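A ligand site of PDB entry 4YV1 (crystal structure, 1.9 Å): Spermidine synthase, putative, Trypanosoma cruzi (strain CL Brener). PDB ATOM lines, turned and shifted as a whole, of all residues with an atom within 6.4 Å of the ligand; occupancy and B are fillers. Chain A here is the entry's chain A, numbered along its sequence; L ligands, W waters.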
ATOM      1  N   PHE A  47     -39.588  11.386   6.624  1.00  0.00           N
ATOM      2  CA  PHE A  47     -38.903  12.679   6.612  1.00  0.00           C
ATOM      3  C   PHE A  47     -38.911  13.524   5.324  1.00  0.00           C
ATOM      4  O   PHE A  47     -38.911  14.745   5.411  1.00  0.00           O
ATOM      5  CB  PHE A  47     -37.469  12.505   7.140  1.00  0.00           C
ATOM      6  CG  PHE A  47     -37.421  12.049   8.577  1.00  0.00           C
ATOM      7  CD1 PHE A  47     -37.689  12.950   9.608  1.00  0.00           C
ATOM      8  CD2 PHE A  47     -37.197  10.725   8.897  1.00  0.00           C
ATOM      9  CE1 PHE A  47     -37.686  12.514  10.937  1.00  0.00           C
ATOM     10  CE2 PHE A  47     -37.193  10.298  10.215  1.00  0.00           C
ATOM     11  CZ  PHE A  47     -37.445  11.175  11.234  1.00  0.00           C
ATOM     12  N   GLN A  48     -38.946  12.893   4.164  1.00  0.00           N
ATOM     13  CA  GLN A  48     -38.831  13.573   2.887  1.00  0.00           C
ATOM     14  C   GLN A  48     -39.392  12.665   1.775  1.00  0.00           C
ATOM     15  O   GLN A  48     -39.623  11.489   1.986  1.00  0.00           O
ATOM     16  CB  GLN A  48     -37.338  13.897   2.605  1.00  0.00           C
ATOM     17  CG  GLN A  48     -36.438  12.688   2.490  1.00  0.00           C
ATOM     18  CD  GLN A  48     -35.023  12.996   2.971  1.00  0.00           C
ATOM     19  OE1 GLN A  48     -34.491  14.093   2.758  1.00  0.00           O
ATOM     20  NE2 GLN A  48     -34.422  12.042   3.675  1.00  0.00           N
ATOM     21  N   MET A  65     -31.155   9.389  -7.889  1.00  0.00           N
ATOM     22  CA  MET A  65     -31.886   9.532  -6.677  1.00  0.00           C
ATOM     23  C   MET A  65     -32.212  10.996  -6.417  1.00  0.00           C
ATOM     24  O   MET A  65     -31.331  11.840  -6.495  1.00  0.00           O
ATOM     25  CB  MET A  65     -31.098   9.017  -5.451  1.00  0.00           C
ATOM     26  CG  MET A  65     -31.824   9.271  -4.137  1.00  0.00           C
ATOM     27  SD  MET A  65     -30.943   8.845  -2.626  1.00  0.00           S
ATOM     28  CE  MET A  65     -30.695   7.117  -2.956  1.00  0.00           C
ATOM     29  N   LEU A  67     -34.447  13.661  -3.587  1.00  0.00           N
ATOM     30  CA  LEU A  67     -35.016  13.851  -2.291  1.00  0.00           C
ATOM     31  C   LEU A  67     -35.740  15.178  -2.335  1.00  0.00           C
ATOM     32  O   LEU A  67     -35.162  16.200  -2.772  1.00  0.00           O
ATOM     33  CB  LEU A  67     -33.982  13.841  -1.135  1.00  0.00           C
ATOM     34  CG  LEU A  67     -33.406  12.507  -0.676  1.00  0.00           C
ATOM     35  CD1 LEU A  67     -32.304  12.759   0.327  1.00  0.00           C
ATOM     36  CD2 LEU A  67     -34.481  11.599  -0.034  1.00  0.00           C
ATOM     37  N   GLN A  72     -29.962  14.217  -5.914  1.00  0.00           N
ATOM     38  CA  GLN A  72     -28.957  14.123  -4.855  1.00  0.00           C
ATOM     39  C   GLN A  72     -27.796  13.277  -5.335  1.00  0.00           C
ATOM     40  O   GLN A  72     -26.655  13.619  -5.056  1.00  0.00           O
ATOM     41  CB  GLN A  72     -29.553  13.584  -3.521  1.00  0.00           C
ATOM     42  CG  GLN A  72     -30.492  14.531  -2.715  1.00  0.00           C
ATOM     43  CD  GLN A  72     -30.001  15.992  -2.497  1.00  0.00           C
ATOM     44  OE1 GLN A  72     -28.808  16.280  -2.334  1.00  0.00           O
ATOM     45  NE2 GLN A  72     -30.958  16.917  -2.481  1.00  0.00           N
ATOM     46  N   VAL A  73     -28.055  12.191  -6.089  1.00  0.00           N
ATOM     47  CA  VAL A  73     -26.958  11.332  -6.573  1.00  0.00           C
ATOM     48  C   VAL A  73     -27.263  10.817  -7.974  1.00  0.00           C
ATOM     49  O   VAL A  73     -28.431  10.558  -8.264  1.00  0.00           O
ATOM     50  CB  VAL A  73     -26.793  10.114  -5.597  1.00  0.00           C
ATOM     51  CG1 VAL A  73     -25.837   9.086  -6.180  1.00  0.00           C
ATOM     52  CG2 VAL A  73     -26.241  10.594  -4.244  1.00  0.00           C
ATOM     53  N   TYR A  81     -18.743  15.114  -5.818  1.00  0.00           N
ATOM     54  CA  TYR A  81     -19.073  15.755  -4.537  1.00  0.00           C
ATOM     55  C   TYR A  81     -18.535  14.819  -3.461  1.00  0.00           C
ATOM     56  O   TYR A  81     -18.081  15.263  -2.421  1.00  0.00           O
ATOM     57  CB  TYR A  81     -20.575  15.874  -4.443  1.00  0.00           C
ATOM     58  CG  TYR A  81     -21.176  16.354  -3.150  1.00  0.00           C
ATOM     59  CD1 TYR A  81     -21.302  17.751  -2.834  1.00  0.00           C
ATOM     60  CD2 TYR A  81     -21.652  15.432  -2.215  1.00  0.00           C
ATOM     61  CE1 TYR A  81     -21.917  18.160  -1.645  1.00  0.00           C
ATOM     62  CE2 TYR A  81     -22.279  15.826  -1.079  1.00  0.00           C
ATOM     63  CZ  TYR A  81     -22.429  17.159  -0.784  1.00  0.00           C
ATOM     64  OH  TYR A  81     -23.037  17.464   0.396  1.00  0.00           O
ATOM     65  N   HIS A  82     -18.576  13.509  -3.679  1.00  0.00           N
ATOM     66  CA  HIS A  82     -18.131  12.571  -2.587  1.00  0.00           C
ATOM     67  C   HIS A  82     -16.611  12.649  -2.365  1.00  0.00           C
ATOM     68  O   HIS A  82     -16.107  12.666  -1.228  1.00  0.00           O
ATOM     69  CB  HIS A  82     -18.617  11.148  -2.924  1.00  0.00           C
ATOM     70  CG  HIS A  82     -20.112  11.033  -2.824  1.00  0.00           C
ATOM     71  ND1 HIS A  82     -20.863  10.239  -3.660  1.00  0.00           N
ATOM     72  CD2 HIS A  82     -20.985  11.702  -2.042  1.00  0.00           C
ATOM     73  CE1 HIS A  82     -22.142  10.394  -3.357  1.00  0.00           C
ATOM     74  NE2 HIS A  82     -22.249  11.293  -2.394  1.00  0.00           N
ATOM     75  N   ILE A 102     -22.543  13.575   9.127  1.00  0.00           N
ATOM     76  CA  ILE A 102     -23.932  13.837   9.394  1.00  0.00           C
ATOM     77  C   ILE A 102     -24.633  13.851   8.052  1.00  0.00           C
ATOM     78  O   ILE A 102     -24.196  14.553   7.146  1.00  0.00           O
ATOM     79  CB  ILE A 102     -24.101  15.194  10.124  1.00  0.00           C
ATOM     80  CG1 ILE A 102     -23.637  15.018  11.592  1.00  0.00           C
ATOM     81  CG2 ILE A 102     -25.613  15.500  10.150  1.00  0.00           C
ATOM     82  CD1 ILE A 102     -23.269  16.264  12.342  1.00  0.00           C
ATOM     83  N   GLY A 103     -25.688  13.071   7.918  1.00  0.00           N
ATOM     84  CA  GLY A 103     -26.349  12.847   6.637  1.00  0.00           C
ATOM     85  C   GLY A 103     -25.614  11.719   5.902  1.00  0.00           C
ATOM     86  O   GLY A 103     -25.298  10.663   6.499  1.00  0.00           O
ATOM     87  N   GLY A 104     -25.390  11.864   4.605  1.00  0.00           N
ATOM     88  CA  GLY A 104     -24.527  10.871   3.966  1.00  0.00           C
ATOM     89  C   GLY A 104     -25.099   9.453   3.845  1.00  0.00           C
ATOM     90  O   GLY A 104     -24.372   8.516   3.623  1.00  0.00           O
ATOM     91  N   GLY A 105     -26.434   9.329   3.948  1.00  0.00           N
ATOM     92  CA  GLY A 105     -27.061   7.992   3.930  1.00  0.00           C
ATOM     93  C   GLY A 105     -26.828   7.136   2.720  1.00  0.00           C
ATOM     94  O   GLY A 105     -26.847   5.926   2.815  1.00  0.00           O
ATOM     95  N   ASP A 106     -26.497   7.749   1.585  1.00  0.00           N
ATOM     96  CA  ASP A 106     -26.141   6.969   0.407  1.00  0.00           C
ATOM     97  C   ASP A 106     -24.829   6.198   0.527  1.00  0.00           C
ATOM     98  O   ASP A 106     -24.625   5.248  -0.203  1.00  0.00           O
ATOM     99  CB  ASP A 106     -26.118   7.890  -0.821  1.00  0.00           C
ATOM    100  CG  ASP A 106     -25.286   9.124  -0.578  1.00  0.00           C
ATOM    101  OD1 ASP A 106     -24.031   9.040  -0.624  1.00  0.00           O
ATOM    102  OD2 ASP A 106     -25.858  10.182  -0.262  1.00  0.00           O
ATOM    103  N   GLY A 107     -23.883   6.664   1.352  1.00  0.00           N
ATOM    104  CA  GLY A 107     -22.686   5.904   1.587  1.00  0.00           C
ATOM    105  C   GLY A 107     -21.505   6.492   0.833  1.00  0.00           C
ATOM    106  O   GLY A 107     -20.399   6.061   1.052  1.00  0.00           O
ATOM    107  N   GLY A 108     -21.720   7.515  -0.006  1.00  0.00           N
ATOM    108  CA  GLY A 108     -20.580   8.015  -0.860  1.00  0.00           C
ATOM    109  C   GLY A 108     -19.443   8.699  -0.121  1.00  0.00           C
ATOM    110  O   GLY A 108     -18.272   8.410  -0.366  1.00  0.00           O
ATOM    111  N   VAL A 109     -19.777   9.619   0.791  1.00  0.00           N
ATOM    112  CA  VAL A 109     -18.719  10.312   1.509  1.00  0.00           C
ATOM    113  C   VAL A 109     -17.990   9.283   2.318  1.00  0.00           C
ATOM    114  O   VAL A 109     -16.771   9.300   2.395  1.00  0.00           O
ATOM    115  CB  VAL A 109     -19.257  11.457   2.396  1.00  0.00           C
ATOM    116  CG1 VAL A 109     -18.134  12.043   3.266  1.00  0.00           C
ATOM    117  CG2 VAL A 109     -19.779  12.610   1.502  1.00  0.00           C
ATOM    118  N   VAL A 125     -24.518   9.386  10.649  1.00  0.00           N
ATOM    119  CA  VAL A 125     -25.844   9.570  11.287  1.00  0.00           C
ATOM    120  C   VAL A 125     -26.733  10.228  10.307  1.00  0.00           C
ATOM    121  O   VAL A 125     -26.547  11.425  10.018  1.00  0.00           O
ATOM    122  CB  VAL A 125     -25.726  10.462  12.554  1.00  0.00           C
ATOM    123  CG1 VAL A 125     -27.109  10.591  13.206  1.00  0.00           C
ATOM    124  CG2 VAL A 125     -24.740   9.862  13.539  1.00  0.00           C
ATOM    125  N   ASP A 126     -27.659   9.463   9.707  1.00  0.00           N
ATOM    126  CA  ASP A 126     -28.591  10.029   8.757  1.00  0.00           C
ATOM    127  C   ASP A 126     -30.022   9.844   9.331  1.00  0.00           C
ATOM    128  O   ASP A 126     -30.354   8.760   9.781  1.00  0.00           O
ATOM    129  CB  ASP A 126     -28.438   9.372   7.334  1.00  0.00           C
ATOM    130  CG  ASP A 126     -29.273  10.080   6.266  1.00  0.00           C
ATOM    131  OD1 ASP A 126     -30.556  10.182   6.434  1.00  0.00           O
ATOM    132  OD2 ASP A 126     -28.650  10.480   5.208  1.00  0.00           O
ATOM    133  N   ILE A 127     -30.820  10.918   9.333  1.00  0.00           N
ATOM    134  CA  ILE A 127     -32.168  10.958   9.943  1.00  0.00           C
ATOM    135  C   ILE A 127     -33.068   9.944   9.267  1.00  0.00           C
ATOM    136  O   ILE A 127     -33.968   9.393   9.914  1.00  0.00           O
ATOM    137  CB  ILE A 127     -32.790  12.387   9.860  1.00  0.00           C
ATOM    138  CG1 ILE A 127     -33.850  12.595  10.965  1.00  0.00           C
ATOM    139  CG2 ILE A 127     -33.288  12.682   8.433  1.00  0.00           C
ATOM    140  CD1 ILE A 127     -34.229  14.043  11.181  1.00  0.00           C
ATOM    141  N   ASP A 128     -32.773   9.650   7.999  1.00  0.00           N
ATOM    142  CA  ASP A 128     -33.661   8.850   7.174  1.00  0.00           C
ATOM    143  C   ASP A 128     -33.131   7.467   6.827  1.00  0.00           C
ATOM    144  O   ASP A 128     -32.403   7.303   5.857  1.00  0.00           O
ATOM    145  CB  ASP A 128     -34.046   9.598   5.898  1.00  0.00           C
ATOM    146  CG  ASP A 128     -35.314   9.004   5.193  1.00  0.00           C
ATOM    147  OD1 ASP A 128     -35.637   7.769   5.291  1.00  0.00           O
ATOM    148  OD2 ASP A 128     -35.954   9.766   4.456  1.00  0.00           O
ATOM    149  N   VAL A 131     -33.293   6.018   3.180  1.00  0.00           N
ATOM    150  CA  VAL A 131     -32.281   6.403   2.208  1.00  0.00           C
ATOM    151  C   VAL A 131     -31.176   5.344   2.166  1.00  0.00           C
ATOM    152  O   VAL A 131     -30.713   4.978   1.083  1.00  0.00           O
ATOM    153  CB  VAL A 131     -31.645   7.787   2.558  1.00  0.00           C
ATOM    154  CG1 VAL A 131     -30.486   8.108   1.578  1.00  0.00           C
ATOM    155  CG2 VAL A 131     -32.716   8.877   2.552  1.00  0.00           C
ATOM    156  N   MET A 132     -30.701   4.913   3.351  1.00  0.00           N
ATOM    157  CA  MET A 132     -29.668   3.869   3.428  1.00  0.00           C
ATOM    158  C   MET A 132     -30.213   2.619   2.760  1.00  0.00           C
ATOM    159  O   MET A 132     -29.500   1.980   1.985  1.00  0.00           O
ATOM    160  CB  MET A 132     -29.283   3.521   4.852  1.00  0.00           C
ATOM    161  CG  MET A 132     -28.283   4.455   5.513  1.00  0.00           C
ATOM    162  SD  MET A 132     -29.214   5.850   6.117  1.00  0.00           S
ATOM    163  CE  MET A 132     -28.927   5.582   7.874  1.00  0.00           C
ATOM    164  N   GLY A 156     -30.895   8.618  12.761  1.00  0.00           N
ATOM    165  CA  GLY A 156     -31.180   9.611  13.762  1.00  0.00           C
ATOM    166  C   GLY A 156     -30.911  10.998  13.216  1.00  0.00           C
ATOM    167  O   GLY A 156     -30.307  11.167  12.147  1.00  0.00           O
ATOM    168  N   ASP A 157     -31.419  11.973  13.957  1.00  0.00           N
ATOM    169  CA  ASP A 157     -31.217  13.366  13.637  1.00  0.00           C
ATOM    170  C   ASP A 157     -29.848  13.797  14.116  1.00  0.00           C
ATOM    171  O   ASP A 157     -29.515  13.707  15.325  1.00  0.00           O
ATOM    172  CB  ASP A 157     -32.320  14.160  14.330  1.00  0.00           C
ATOM    173  CG  ASP A 157     -32.262  15.651  14.060  1.00  0.00           C
ATOM    174  OD1 ASP A 157     -31.283  16.205  13.485  1.00  0.00           O
ATOM    175  OD2 ASP A 157     -33.221  16.295  14.491  1.00  0.00           O
ATOM    176  N   GLY A 158     -29.057  14.332  13.175  1.00  0.00           N
ATOM    177  CA  GLY A 158     -27.728  14.819  13.541  1.00  0.00           C
ATOM    178  C   GLY A 158     -27.700  15.898  14.585  1.00  0.00           C
ATOM    179  O   GLY A 158     -26.745  16.000  15.372  1.00  0.00           O
ATOM    180  N   LEU A 159     -28.724  16.746  14.587  1.00  0.00           N
ATOM    181  CA  LEU A 159     -28.779  17.821  15.607  1.00  0.00           C
ATOM    182  C   LEU A 159     -28.727  17.229  17.053  1.00  0.00           C
ATOM    183  O   LEU A 159     -27.947  17.690  17.920  1.00  0.00           O
ATOM    184  CB  LEU A 159     -30.046  18.652  15.399  1.00  0.00           C
ATOM    185  CG  LEU A 159     -30.154  20.035  16.039  1.00  0.00           C
ATOM    186  CD1 LEU A 159     -29.321  21.044  15.266  1.00  0.00           C
ATOM    187  CD2 LEU A 159     -31.622  20.423  16.016  1.00  0.00           C
ATOM    188  N   ASP A 176     -23.006  16.339   5.169  1.00  0.00           N
ATOM    189  CA  ASP A 176     -23.522  16.017   3.837  1.00  0.00           C
ATOM    190  C   ASP A 176     -25.040  15.958   3.911  1.00  0.00           C
ATOM    191  O   ASP A 176     -25.665  14.893   3.865  1.00  0.00           O
ATOM    192  CB  ASP A 176     -22.948  14.684   3.412  1.00  0.00           C
ATOM    193  CG  ASP A 176     -23.454  14.251   2.064  1.00  0.00           C
ATOM    194  OD1 ASP A 176     -23.911  15.158   1.347  1.00  0.00           O
ATOM    195  OD2 ASP A 176     -23.464  13.018   1.763  1.00  0.00           O
ATOM    196  N   THR A 177     -25.626  17.130   3.986  1.00  0.00           N
ATOM    197  CA  THR A 177     -27.071  17.275   4.066  1.00  0.00           C
ATOM    198  C   THR A 177     -27.759  17.787   2.771  1.00  0.00           C
ATOM    199  O   THR A 177     -27.117  18.322   1.828  1.00  0.00           O
ATOM    200  CB  THR A 177     -27.450  18.336   5.099  1.00  0.00           C
ATOM    201  OG1 THR A 177     -26.687  19.530   4.795  1.00  0.00           O
ATOM    202  CG2 THR A 177     -27.187  17.842   6.474  1.00  0.00           C
ATOM    203  N   THR A 178     -29.098  17.653   2.788  1.00  0.00           N
ATOM    204  CA  THR A 178     -30.002  18.110   1.719  1.00  0.00           C
ATOM    205  C   THR A 178     -30.011  19.635   1.470  1.00  0.00           C
ATOM    206  O   THR A 178     -30.045  20.417   2.413  1.00  0.00           O
ATOM    207  CB  THR A 178     -31.431  17.611   2.022  1.00  0.00           C
ATOM    208  OG1 THR A 178     -31.638  17.551   3.456  1.00  0.00           O
ATOM    209  CG2 THR A 178     -31.574  16.200   1.480  1.00  0.00           C
ATOM    210  N   GLN A 209     -22.200  20.951   3.150  1.00  0.00           N
ATOM    211  CA  GLN A 209     -22.761  21.035   1.807  1.00  0.00           C
ATOM    212  C   GLN A 209     -22.959  22.518   1.691  1.00  0.00           C
ATOM    213  O   GLN A 209     -23.646  23.105   2.505  1.00  0.00           O
ATOM    214  CB  GLN A 209     -24.064  20.222   1.765  1.00  0.00           C
ATOM    215  CG  GLN A 209     -24.683  19.983   0.364  1.00  0.00           C
ATOM    216  CD  GLN A 209     -25.629  21.097  -0.041  1.00  0.00           C
ATOM    217  OE1 GLN A 209     -26.840  21.049   0.267  1.00  0.00           O
ATOM    218  NE2 GLN A 209     -25.097  22.119  -0.738  1.00  0.00           N
ATOM    219  N   TYR A 245     -26.227  19.286 -10.589  1.00  0.00           N
ATOM    220  CA  TYR A 245     -26.752  20.169  -9.568  1.00  0.00           C
ATOM    221  C   TYR A 245     -27.121  21.478 -10.250  1.00  0.00           C
ATOM    222  O   TYR A 245     -26.564  21.800 -11.323  1.00  0.00           O
ATOM    223  CB  TYR A 245     -25.742  20.356  -8.404  1.00  0.00           C
ATOM    224  CG  TYR A 245     -25.614  19.141  -7.435  1.00  0.00           C
ATOM    225  CD1 TYR A 245     -26.598  18.134  -7.345  1.00  0.00           C
ATOM    226  CD2 TYR A 245     -24.509  19.027  -6.568  1.00  0.00           C
ATOM    227  CE1 TYR A 245     -26.463  17.043  -6.446  1.00  0.00           C
ATOM    228  CE2 TYR A 245     -24.377  17.952  -5.672  1.00  0.00           C
ATOM    229  CZ  TYR A 245     -25.358  16.968  -5.589  1.00  0.00           C
ATOM    230  OH  TYR A 245     -25.186  15.925  -4.674  1.00  0.00           O
HETATM  231  C1  LIG L   1     -24.964  13.578  -1.507  1.00  0.00           C
HETATM  232  N1  LIG L   1     -24.462  12.322  -0.842  1.00  0.00           N
HETATM  233  C2  LIG L   1     -26.481  13.688  -1.286  1.00  0.00           C
HETATM  234  C3  LIG L   1     -26.852  14.301   0.035  1.00  0.00           C
HETATM  235  S1  LIG L   1     -27.440  13.008   1.203  1.00  0.00           S
HETATM  236  C4  LIG L   1     -28.659  12.066   0.196  1.00  0.00           C
HETATM  237  C5  LIG L   1     -28.535  14.145   2.126  1.00  0.00           C
HETATM  238  C6  LIG L   1     -28.844  13.425   3.469  1.00  0.00           C
HETATM  239  O1  LIG L   1     -28.957  14.297   4.600  1.00  0.00           O
HETATM  240  C7  LIG L   1     -29.943  13.660   5.435  1.00  0.00           C
HETATM  241  C8  LIG L   1     -31.020  13.232   4.433  1.00  0.00           C
HETATM  242  O2  LIG L   1     -31.887  12.227   4.978  1.00  0.00           O
HETATM  243  C9  LIG L   1     -30.182  12.737   3.254  1.00  0.00           C
HETATM  244  O3  LIG L   1     -29.938  11.329   3.140  1.00  0.00           O
HETATM  245  N2  LIG L   1     -30.395  14.529   6.512  1.00  0.00           N
HETATM  246  C10 LIG L   1     -31.234  15.616   6.399  1.00  0.00           C
HETATM  247  N3  LIG L   1     -31.436  16.190   7.571  1.00  0.00           N
HETATM  248  C11 LIG L   1     -30.713  15.472   8.494  1.00  0.00           C
HETATM  249  C12 LIG L   1     -30.546  15.595   9.870  1.00  0.00           C
HETATM  250  N4  LIG L   1     -31.125  16.593  10.689  1.00  0.00           N
HETATM  251  C13 LIG L   1     -30.056  14.441   7.848  1.00  0.00           C
HETATM  252  N5  LIG L   1     -29.281  13.526   8.416  1.00  0.00           N
HETATM  253  C14 LIG L   1     -29.173  13.755   9.706  1.00  0.00           C
HETATM  254  N6  LIG L   1     -29.744  14.698  10.464  1.00  0.00           N
HETATM  255  O   HOH W   1     -22.591  10.615   1.248  1.00  0.00           O
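Residues that only touch the ligand: Leu 67, Gln 72, Tyr 81, Ile 102, Gly 103, Gly 104, Val 125, Asp 128, Val 131, Gly 156, Thr 177, Thr 178 and Tyr 245. Hydrophobic or aromatic side chains within 4 Å of the ligand: Leu 67, Tyr 81, His 82, Ile 102, Ile 127 and Val 131. Of the 31 residues printed, 21 come within 4 Å of the ligand.
The backbone NH (N) of Gly 156 is in hydrogen-bond range of the backbone carbonyl oxygen (O) of Asp 126, 3.0 Å away. The backbone NH (N) of Gly 108 sits at hydrogen-bond distance from the side-chain carboxylate (OD1) of Asp 106 (2.8 Å). OD1 of Asp 157 is in hydrogen-bond range of N of Leu 159 (2.8 Å). The side-chain carboxylate (OD2) of Asp 128 lies within hydrogen-bond range of the side-chain amide nitrogen (NE2) of Gln 48 (2.9 Å). The backbone NH of Asp 176 lies within hydrogen-bond range of the backbone carbonyl oxygen of Ile 102, at 2.9 Å. O of Gly 156 sits at hydrogen-bond distance from N of Ile 127 (2.9 Å). O of Thr 177 lies close to OE1 of Gln 209, 3.2 Å away. The backbone carbonyl oxygen of Gln 72 lies within hydrogen-bond range of the side-chain hydroxyl of Tyr 245 (2.8 Å).
An oxygen (O3) of the ligand is in hydrogen-bond range of the side-chain carboxylate (OD2) of Asp 126 (2.6 Å). N1 of the ligand lies within salt-bridge range of OD2 of Asp 106 (2.6 Å). N of Gly 158 is in hydrogen-bond range of N6 of the ligand (2.8 Å). A nitrogen (N4) of the ligand is in hydrogen-bond range of the side-chain carboxylate (OD1) of Asp 157 (2.8 Å). NE2 of Gln 48 sits at hydrogen-bond distance from O2 of the ligand, 2.9 Å away. The backbone carbonyl oxygen of Asp 176 lies close to a sulfur (S1) of the ligand, at 3.7 Å. A nitrogen (N1) of the ligand lies within salt-bridge range of the side-chain carboxylate (OD2) of Asp 176 (2.9 Å). N1 of the ligand is in hydrogen-bond range of NE2 of His 82, at 2.9 Å. The backbone NH (N) of Ile 127 sits at hydrogen-bond distance from a nitrogen (N5) of the ligand.
Water W1 lies within hydrogen-bond range of the side-chain carboxylate (OD2) of Asp 176 (2.6 Å), the side-chain carboxylate (OD1) of Asp 106 (2.8 Å), the backbone NH (N) of Val 109 (3.0 Å), a nitrogen (N1) of the ligand (3.3 Å) and the backbone NH (N) of Gly 108 (3.5 Å).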
